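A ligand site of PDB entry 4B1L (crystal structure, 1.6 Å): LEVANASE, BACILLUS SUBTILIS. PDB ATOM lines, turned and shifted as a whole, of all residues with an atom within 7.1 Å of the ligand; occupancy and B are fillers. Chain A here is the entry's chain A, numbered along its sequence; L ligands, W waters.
The side-chain carboxylate of Asp 82 sits at hydrogen-bond distance from an oxygen (O6) of the ligand, 2.7 Å away. The side-chain amino group (NZ) of Lys 89 sits at hydrogen-bond distance from an oxygen (O5) of the ligand (2.8 Å). O6 of the ligand lies within hydrogen-bond range of ND2 of Asn 80, 3.1 Å away. The side-chain carboxylate (OD1) of Asp 34 lies within hydrogen-bond range of an oxygen (O4) of the ligand (2.5 Å).
OD2 of Asp 82 is in hydrogen-bond range of ND1 of His 85 (2.7 Å). N of Asn 80 is in hydrogen-bond range of O of Lys 89 (2.9 Å). O of Ala 62 is in hydrogen-bond range of N of Trp 152 (2.9 Å). O of Leu 87 lies within hydrogen-bond range of N of Asp 82. N of Leu 78 is in hydrogen-bond range of O of Phe 91 (2.8 Å). The side-chain carboxylate (OD1) of Asp 34 is in hydrogen-bond range of the side-chain amide nitrogen (ND2) of Asn 150, 3.1 Å away.
Residues that only touch the ligand: Ala 62, Phe 91, Ala 98, Val 100 and Trp 152. Hydrophobic or aromatic side chains within 4 Å of the ligand: Ala 62, Phe 91, Ala 98, Val 100 and Trp 152. Of the 27 residues printed, 9 come within 4 Å of the ligand. The nearest printed residue that does not touch the ligand is Asn 150 (4.4 Å).
Water W1 lies within hydrogen-bond range of the side-chain amide oxygen of Asn 150 (2.8 Å), an oxygen (O4) of the ligand (2.9 Å) and the side-chain amide nitrogen of Asn 80 (3.1 Å).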
ATOM      1  N   GLY A  33      -8.939   3.705 -29.656  1.00  0.00           N
ATOM      2  CA  GLY A  33      -8.304   2.744 -28.745  1.00  0.00           C
ATOM      3  C   GLY A  33      -7.324   3.414 -27.790  1.00  0.00           C
ATOM      4  O   GLY A  33      -7.273   4.667 -27.661  1.00  0.00           O
ATOM      5  N   ASP A  34      -6.552   2.573 -27.128  1.00  0.00           N
ATOM      6  CA  ASP A  34      -5.573   2.996 -26.140  1.00  0.00           C
ATOM      7  C   ASP A  34      -4.287   3.547 -26.738  1.00  0.00           C
ATOM      8  O   ASP A  34      -3.681   2.943 -27.624  1.00  0.00           O
ATOM      9  CB  ASP A  34      -5.206   1.829 -25.230  1.00  0.00           C
ATOM     10  CG  ASP A  34      -6.269   1.508 -24.204  1.00  0.00           C
ATOM     11  OD1 ASP A  34      -6.697   2.416 -23.486  1.00  0.00           O
ATOM     12  OD2 ASP A  34      -6.676   0.335 -24.106  1.00  0.00           O
ATOM     13  N   SER A  35      -3.852   4.687 -26.191  1.00  0.00           N
ATOM     14  CA  SER A  35      -2.530   5.192 -26.524  1.00  0.00           C
ATOM     15  C   SER A  35      -1.824   5.751 -25.288  1.00  0.00           C
ATOM     16  O   SER A  35      -2.469   5.990 -24.257  1.00  0.00           O
ATOM     17  CB  SER A  35      -2.625   6.276 -27.628  1.00  0.00           C
ATOM     18  OG  SER A  35      -3.382   7.422 -27.167  1.00  0.00           O
ATOM     19  N   PHE A  36      -0.505   5.931 -25.403  1.00  0.00           N
ATOM     20  CA  PHE A  36       0.338   6.137 -24.221  1.00  0.00           C
ATOM     21  C   PHE A  36       1.474   7.095 -24.481  1.00  0.00           C
ATOM     22  O   PHE A  36       2.043   7.109 -25.568  1.00  0.00           O
ATOM     23  CB  PHE A  36       0.958   4.823 -23.745  1.00  0.00           C
ATOM     24  CG  PHE A  36      -0.023   3.709 -23.558  1.00  0.00           C
ATOM     25  CD1 PHE A  36      -0.306   2.858 -24.618  1.00  0.00           C
ATOM     26  CD2 PHE A  36      -0.599   3.451 -22.307  1.00  0.00           C
ATOM     27  CE1 PHE A  36      -1.211   1.837 -24.472  1.00  0.00           C
ATOM     28  CE2 PHE A  36      -1.499   2.395 -22.163  1.00  0.00           C
ATOM     29  CZ  PHE A  36      -1.794   1.588 -23.250  1.00  0.00           C
ATOM     30  N   GLY A  61     -14.268   8.897 -24.864  1.00  0.00           N
ATOM     31  CA  GLY A  61     -13.972   7.795 -23.947  1.00  0.00           C
ATOM     32  C   GLY A  61     -13.302   8.268 -22.665  1.00  0.00           C
ATOM     33  O   GLY A  61     -13.942   8.880 -21.819  1.00  0.00           O
ATOM     34  N   ALA A  62     -12.014   7.955 -22.520  1.00  0.00           N
ATOM     35  CA  ALA A  62     -11.303   8.048 -21.231  1.00  0.00           C
ATOM     36  C   ALA A  62      -9.924   8.726 -21.307  1.00  0.00           C
ATOM     37  O   ALA A  62      -9.261   8.716 -22.367  1.00  0.00           O
ATOM     38  CB  ALA A  62     -11.131   6.646 -20.642  1.00  0.00           C
ATOM     39  N   GLY A  63      -9.495   9.255 -20.165  1.00  0.00           N
ATOM     40  CA  GLY A  63      -8.120   9.728 -19.970  1.00  0.00           C
ATOM     41  C   GLY A  63      -7.597   9.157 -18.660  1.00  0.00           C
ATOM     42  O   GLY A  63      -8.369   9.039 -17.718  1.00  0.00           O
ATOM     43  N   ALA A  64      -6.296   8.833 -18.617  1.00  0.00           N
ATOM     44  CA  ALA A  64      -5.716   8.047 -17.523  1.00  0.00           C
ATOM     45  C   ALA A  64      -4.346   8.463 -17.089  1.00  0.00           C
ATOM     46  O   ALA A  64      -3.495   8.908 -17.912  1.00  0.00           O
ATOM     47  CB  ALA A  64      -5.650   6.564 -17.935  1.00  0.00           C
ATOM     48  N   LEU A  78      -3.094   1.688 -14.372  1.00  0.00           N
ATOM     49  CA  LEU A  78      -3.739   2.938 -14.773  1.00  0.00           C
ATOM     50  C   LEU A  78      -4.886   3.237 -13.801  1.00  0.00           C
ATOM     51  O   LEU A  78      -5.555   2.330 -13.233  1.00  0.00           O
ATOM     52  CB  LEU A  78      -4.263   2.866 -16.244  1.00  0.00           C
ATOM     53  CG  LEU A  78      -3.179   2.781 -17.342  1.00  0.00           C
ATOM     54  CD1 LEU A  78      -2.677   1.374 -17.583  1.00  0.00           C
ATOM     55  CD2 LEU A  78      -3.668   3.394 -18.644  1.00  0.00           C
ATOM     56  N   ASN A  80      -8.319   5.858 -14.312  1.00  0.00           N
ATOM     57  CA  ASN A  80      -8.902   6.746 -15.329  1.00  0.00           C
ATOM     58  C   ASN A  80     -10.203   7.405 -14.953  1.00  0.00           C
ATOM     59  O   ASN A  80     -10.765   7.087 -13.890  1.00  0.00           O
ATOM     60  CB  ASN A  80      -8.996   6.035 -16.712  1.00  0.00           C
ATOM     61  CG  ASN A  80     -10.165   5.071 -16.827  1.00  0.00           C
ATOM     62  OD1 ASN A  80     -11.021   4.937 -15.927  1.00  0.00           O
ATOM     63  ND2 ASN A  80     -10.222   4.398 -17.955  1.00  0.00           N
ATOM     64  N   VAL A  81     -10.621   8.377 -15.778  1.00  0.00           N
ATOM     65  CA  VAL A  81     -12.015   8.827 -15.827  1.00  0.00           C
ATOM     66  C   VAL A  81     -12.509   8.492 -17.223  1.00  0.00           C
ATOM     67  O   VAL A  81     -11.824   8.733 -18.238  1.00  0.00           O
ATOM     68  CB  VAL A  81     -12.210  10.352 -15.493  1.00  0.00           C
ATOM     69  CG1 VAL A  81     -11.897  10.622 -14.025  1.00  0.00           C
ATOM     70  CG2 VAL A  81     -11.411  11.280 -16.446  1.00  0.00           C
ATOM     71  N   ASP A  82     -13.689   7.854 -17.259  1.00  0.00           N
ATOM     72  CA  ASP A  82     -14.274   7.352 -18.500  1.00  0.00           C
ATOM     73  C   ASP A  82     -15.627   8.003 -18.630  1.00  0.00           C
ATOM     74  O   ASP A  82     -16.561   7.631 -17.903  1.00  0.00           O
ATOM     75  CB  ASP A  82     -14.411   5.821 -18.411  1.00  0.00           C
ATOM     76  CG  ASP A  82     -14.913   5.198 -19.707  1.00  0.00           C
ATOM     77  OD1 ASP A  82     -15.675   5.866 -20.459  1.00  0.00           O
ATOM     78  OD2 ASP A  82     -14.548   4.018 -19.980  1.00  0.00           O
ATOM     79  N   HIS A  85     -18.537   5.585 -20.258  1.00  0.00           N
ATOM     80  CA  HIS A  85     -19.044   4.559 -19.344  1.00  0.00           C
ATOM     81  C   HIS A  85     -19.376   5.041 -17.975  1.00  0.00           C
ATOM     82  O   HIS A  85     -19.908   4.271 -17.171  1.00  0.00           O
ATOM     83  CB  HIS A  85     -18.059   3.369 -19.293  1.00  0.00           C
ATOM     84  CG  HIS A  85     -17.799   2.799 -20.644  1.00  0.00           C
ATOM     85  ND1 HIS A  85     -16.586   2.856 -21.234  1.00  0.00           N
ATOM     86  CD2 HIS A  85     -18.660   2.214 -21.582  1.00  0.00           C
ATOM     87  CE1 HIS A  85     -16.664   2.309 -22.451  1.00  0.00           C
ATOM     88  NE2 HIS A  85     -17.922   1.925 -22.672  1.00  0.00           N
ATOM     89  N   LEU A  87     -17.390   5.931 -15.355  1.00  0.00           N
ATOM     90  CA  LEU A  87     -16.605   5.074 -14.493  1.00  0.00           C
ATOM     91  C   LEU A  87     -15.308   5.735 -14.159  1.00  0.00           C
ATOM     92  O   LEU A  87     -14.755   6.484 -14.972  1.00  0.00           O
ATOM     93  CB  LEU A  87     -16.267   3.737 -15.174  1.00  0.00           C
ATOM     94  CG  LEU A  87     -17.376   2.685 -15.206  1.00  0.00           C
ATOM     95  CD1 LEU A  87     -16.921   1.502 -16.053  1.00  0.00           C
ATOM     96  CD2 LEU A  87     -17.741   2.257 -13.780  1.00  0.00           C
ATOM     97  N   LYS A  89     -11.889   3.909 -13.267  1.00  0.00           N
ATOM     98  CA  LYS A  89     -11.350   2.522 -13.232  1.00  0.00           C
ATOM     99  C   LYS A  89      -9.955   2.530 -12.678  1.00  0.00           C
ATOM    100  O   LYS A  89      -9.202   3.454 -12.936  1.00  0.00           O
ATOM    101  CB  LYS A  89     -11.285   1.861 -14.635  1.00  0.00           C
ATOM    102  CG  LYS A  89     -12.614   1.587 -15.290  1.00  0.00           C
ATOM    103  CD  LYS A  89     -12.358   0.838 -16.607  1.00  0.00           C
ATOM    104  CE  LYS A  89     -13.644   0.508 -17.354  1.00  0.00           C
ATOM    105  NZ  LYS A  89     -13.260  -0.072 -18.647  1.00  0.00           N
ATOM    106  N   PHE A  91      -7.002  -0.162 -13.139  1.00  0.00           N
ATOM    107  CA  PHE A  91      -6.748  -1.325 -13.981  1.00  0.00           C
ATOM    108  C   PHE A  91      -5.254  -1.513 -14.274  1.00  0.00           C
ATOM    109  O   PHE A  91      -4.406  -0.694 -13.869  1.00  0.00           O
ATOM    110  CB  PHE A  91      -7.665  -1.282 -15.242  1.00  0.00           C
ATOM    111  CG  PHE A  91      -7.416  -0.135 -16.214  1.00  0.00           C
ATOM    112  CD1 PHE A  91      -7.864   1.172 -15.919  1.00  0.00           C
ATOM    113  CD2 PHE A  91      -6.773  -0.358 -17.416  1.00  0.00           C
ATOM    114  CE1 PHE A  91      -7.724   2.190 -16.826  1.00  0.00           C
ATOM    115  CE2 PHE A  91      -6.609   0.692 -18.332  1.00  0.00           C
ATOM    116  CZ  PHE A  91      -7.089   1.957 -18.036  1.00  0.00           C
ATOM    117  N   LYS A  92      -4.936  -2.618 -14.937  1.00  0.00           N
ATOM    118  CA  LYS A  92      -3.562  -2.949 -15.268  1.00  0.00           C
ATOM    119  C   LYS A  92      -3.451  -3.510 -16.678  1.00  0.00           C
ATOM    120  O   LYS A  92      -4.341  -4.160 -17.162  1.00  0.00           O
ATOM    121  CB  LYS A  92      -3.012  -3.954 -14.247  1.00  0.00           C
ATOM    122  CG  LYS A  92      -3.743  -5.286 -14.203  1.00  0.00           C
ATOM    123  CD  LYS A  92      -3.064  -6.268 -13.245  1.00  0.00           C
ATOM    124  CE  LYS A  92      -3.783  -7.613 -13.183  1.00  0.00           C
ATOM    125  NZ  LYS A  92      -3.601  -8.370 -14.471  1.00  0.00           N
ATOM    126  N   PHE A  93      -2.342  -3.210 -17.323  1.00  0.00           N
ATOM    127  CA  PHE A  93      -1.919  -3.973 -18.502  1.00  0.00           C
ATOM    128  C   PHE A  93      -0.936  -5.016 -18.042  1.00  0.00           C
ATOM    129  O   PHE A  93      -0.075  -4.737 -17.233  1.00  0.00           O
ATOM    130  CB  PHE A  93      -1.261  -3.049 -19.507  1.00  0.00           C
ATOM    131  CG  PHE A  93      -2.244  -2.355 -20.398  1.00  0.00           C
ATOM    132  CD1 PHE A  93      -2.802  -1.152 -20.016  1.00  0.00           C
ATOM    133  CD2 PHE A  93      -2.623  -2.939 -21.613  1.00  0.00           C
ATOM    134  CE1 PHE A  93      -3.737  -0.511 -20.840  1.00  0.00           C
ATOM    135  CE2 PHE A  93      -3.549  -2.302 -22.440  1.00  0.00           C
ATOM    136  CZ  PHE A  93      -4.121  -1.091 -22.042  1.00  0.00           C
ATOM    137  N   ALA A  97      -2.252  -6.528 -22.467  1.00  0.00           N
ATOM    138  CA  ALA A  97      -3.716  -6.429 -22.434  1.00  0.00           C
ATOM    139  C   ALA A  97      -4.246  -5.975 -21.083  1.00  0.00           C
ATOM    140  O   ALA A  97      -3.652  -6.259 -20.038  1.00  0.00           O
ATOM    141  CB  ALA A  97      -4.368  -7.726 -22.829  1.00  0.00           C
ATOM    142  N   ALA A  98      -5.388  -5.297 -21.103  1.00  0.00           N
ATOM    143  CA  ALA A  98      -5.954  -4.646 -19.910  1.00  0.00           C
ATOM    144  C   ALA A  98      -6.871  -5.594 -19.168  1.00  0.00           C
ATOM    145  O   ALA A  98      -7.562  -6.415 -19.775  1.00  0.00           O
ATOM    146  CB  ALA A  98      -6.750  -3.423 -20.327  1.00  0.00           C
ATOM    147  N   SER A  99      -6.858  -5.462 -17.839  1.00  0.00           N
ATOM    148  CA  SER A  99      -7.870  -6.110 -16.995  1.00  0.00           C
ATOM    149  C   SER A  99      -8.109  -5.201 -15.803  1.00  0.00           C
ATOM    150  O   SER A  99      -7.212  -4.474 -15.364  1.00  0.00           O
ATOM    151  CB  SER A  99      -7.508  -7.548 -16.599  1.00  0.00           C
ATOM    152  OG  SER A  99      -6.557  -7.600 -15.567  1.00  0.00           O
ATOM    153  N   VAL A 100      -9.336  -5.222 -15.294  1.00  0.00           N
ATOM    154  CA  VAL A 100      -9.726  -4.199 -14.322  1.00  0.00           C
ATOM    155  C   VAL A 100      -9.682  -4.747 -12.908  1.00  0.00           C
ATOM    156  O   VAL A 100     -10.075  -5.904 -12.675  1.00  0.00           O
ATOM    157  CB  VAL A 100     -11.112  -3.628 -14.676  1.00  0.00           C
ATOM    158  CG1 VAL A 100     -11.517  -2.539 -13.677  1.00  0.00           C
ATOM    159  CG2 VAL A 100     -11.076  -3.095 -16.111  1.00  0.00           C
ATOM    160  N   GLU A 103     -13.590  -0.563  -9.992  1.00  0.00           N
ATOM    161  CA  GLU A 103     -14.245   0.494 -10.777  1.00  0.00           C
ATOM    162  C   GLU A 103     -15.395   1.086  -9.965  1.00  0.00           C
ATOM    163  O   GLU A 103     -16.108   0.364  -9.261  1.00  0.00           O
ATOM    164  CB  GLU A 103     -14.722  -0.002 -12.169  1.00  0.00           C
ATOM    165  CG  GLU A 103     -15.709  -1.154 -12.098  1.00  0.00           C
ATOM    166  CD  GLU A 103     -15.846  -1.922 -13.398  1.00  0.00           C
ATOM    167  OE1 GLU A 103     -14.975  -2.753 -13.722  1.00  0.00           O
ATOM    168  OE2 GLU A 103     -16.862  -1.737 -14.071  1.00  0.00           O
ATOM    169  N   ASN A 150      -2.422   8.220 -20.522  1.00  0.00           N
ATOM    170  CA  ASN A 150      -3.130   7.434 -21.542  1.00  0.00           C
ATOM    171  C   ASN A 150      -4.463   8.084 -21.949  1.00  0.00           C
ATOM    172  O   ASN A 150      -5.087   8.778 -21.164  1.00  0.00           O
ATOM    173  CB  ASN A 150      -3.259   5.948 -21.102  1.00  0.00           C
ATOM    174  CG  ASN A 150      -4.546   5.280 -21.579  1.00  0.00           C
ATOM    175  OD1 ASN A 150      -5.639   5.718 -21.210  1.00  0.00           O
ATOM    176  ND2 ASN A 150      -4.430   4.211 -22.410  1.00  0.00           N
ATOM    177  N   VAL A 151      -4.870   7.902 -23.197  1.00  0.00           N
ATOM    178  CA  VAL A 151      -6.280   8.137 -23.584  1.00  0.00           C
ATOM    179  C   VAL A 151      -6.835   6.883 -24.265  1.00  0.00           C
ATOM    180  O   VAL A 151      -6.078   6.082 -24.824  1.00  0.00           O
ATOM    181  CB  VAL A 151      -6.485   9.407 -24.450  1.00  0.00           C
ATOM    182  CG1 VAL A 151      -5.892  10.663 -23.795  1.00  0.00           C
ATOM    183  CG2 VAL A 151      -5.881   9.234 -25.842  1.00  0.00           C
ATOM    184  N   TRP A 152      -8.150   6.708 -24.173  1.00  0.00           N
ATOM    185  CA  TRP A 152      -8.844   5.600 -24.789  1.00  0.00           C
ATOM    186  C   TRP A 152     -10.047   6.124 -25.549  1.00  0.00           C
ATOM    187  O   TRP A 152     -10.954   6.718 -24.963  1.00  0.00           O
ATOM    188  CB  TRP A 152      -9.217   4.528 -23.746  1.00  0.00           C
ATOM    189  CG  TRP A 152     -10.074   3.510 -24.437  1.00  0.00           C
ATOM    190  CD1 TRP A 152      -9.652   2.501 -25.314  1.00  0.00           C
ATOM    191  CD2 TRP A 152     -11.534   3.502 -24.502  1.00  0.00           C
ATOM    192  NE1 TRP A 152     -10.737   1.840 -25.829  1.00  0.00           N
ATOM    193  CE2 TRP A 152     -11.898   2.378 -25.368  1.00  0.00           C
ATOM    194  CE3 TRP A 152     -12.559   4.234 -23.848  1.00  0.00           C
ATOM    195  CZ2 TRP A 152     -13.242   2.045 -25.630  1.00  0.00           C
ATOM    196  CZ3 TRP A 152     -13.905   3.889 -24.131  1.00  0.00           C
ATOM    197  CH2 TRP A 152     -14.230   2.814 -24.990  1.00  0.00           C
ATOM    198  N   ASP A 153     -10.063   5.929 -26.866  1.00  0.00           N
ATOM    199  CA  ASP A 153     -11.178   6.399 -27.725  1.00  0.00           C
ATOM    200  C   ASP A 153     -11.571   7.823 -27.377  1.00  0.00           C
ATOM    201  O   ASP A 153     -12.755   8.112 -27.143  1.00  0.00           O
ATOM    202  CB  ASP A 153     -12.400   5.510 -27.529  1.00  0.00           C
ATOM    203  CG  ASP A 153     -12.509   4.436 -28.560  1.00  0.00           C
ATOM    204  OD1 ASP A 153     -11.512   4.093 -29.258  1.00  0.00           O
ATOM    205  OD2 ASP A 153     -13.637   3.899 -28.650  1.00  0.00           O
HETATM  206  C1  LIG L   1     -10.178  -1.728 -19.741  1.00  0.00           C
HETATM  207  C2  LIG L   1     -10.360  -0.700 -20.875  1.00  0.00           C
HETATM  208  C3  LIG L   1      -9.043  -0.121 -21.432  1.00  0.00           C
HETATM  209  C4  LIG L   1      -9.380   1.378 -21.601  1.00  0.00           C
HETATM  210  C5  LIG L   1     -10.367   1.604 -20.466  1.00  0.00           C
HETATM  211  C6  LIG L   1     -11.398   2.691 -20.714  1.00  0.00           C
HETATM  212  O1  LIG L   1     -11.456  -2.258 -19.383  1.00  0.00           O
HETATM  213  O2  LIG L   1     -11.119  -1.240 -21.939  1.00  0.00           O
HETATM  214  O3  LIG L   1      -8.648  -0.719 -22.675  1.00  0.00           O
HETATM  215  O4  LIG L   1      -8.209   2.158 -21.464  1.00  0.00           O
HETATM  216  O5  LIG L   1     -11.120   0.378 -20.370  1.00  0.00           O
HETATM  217  O6  LIG L   1     -12.240   2.663 -19.551  1.00  0.00           O
HETATM  218  O   HOH W   1      -8.058   4.693 -20.139  1.00  0.00           O
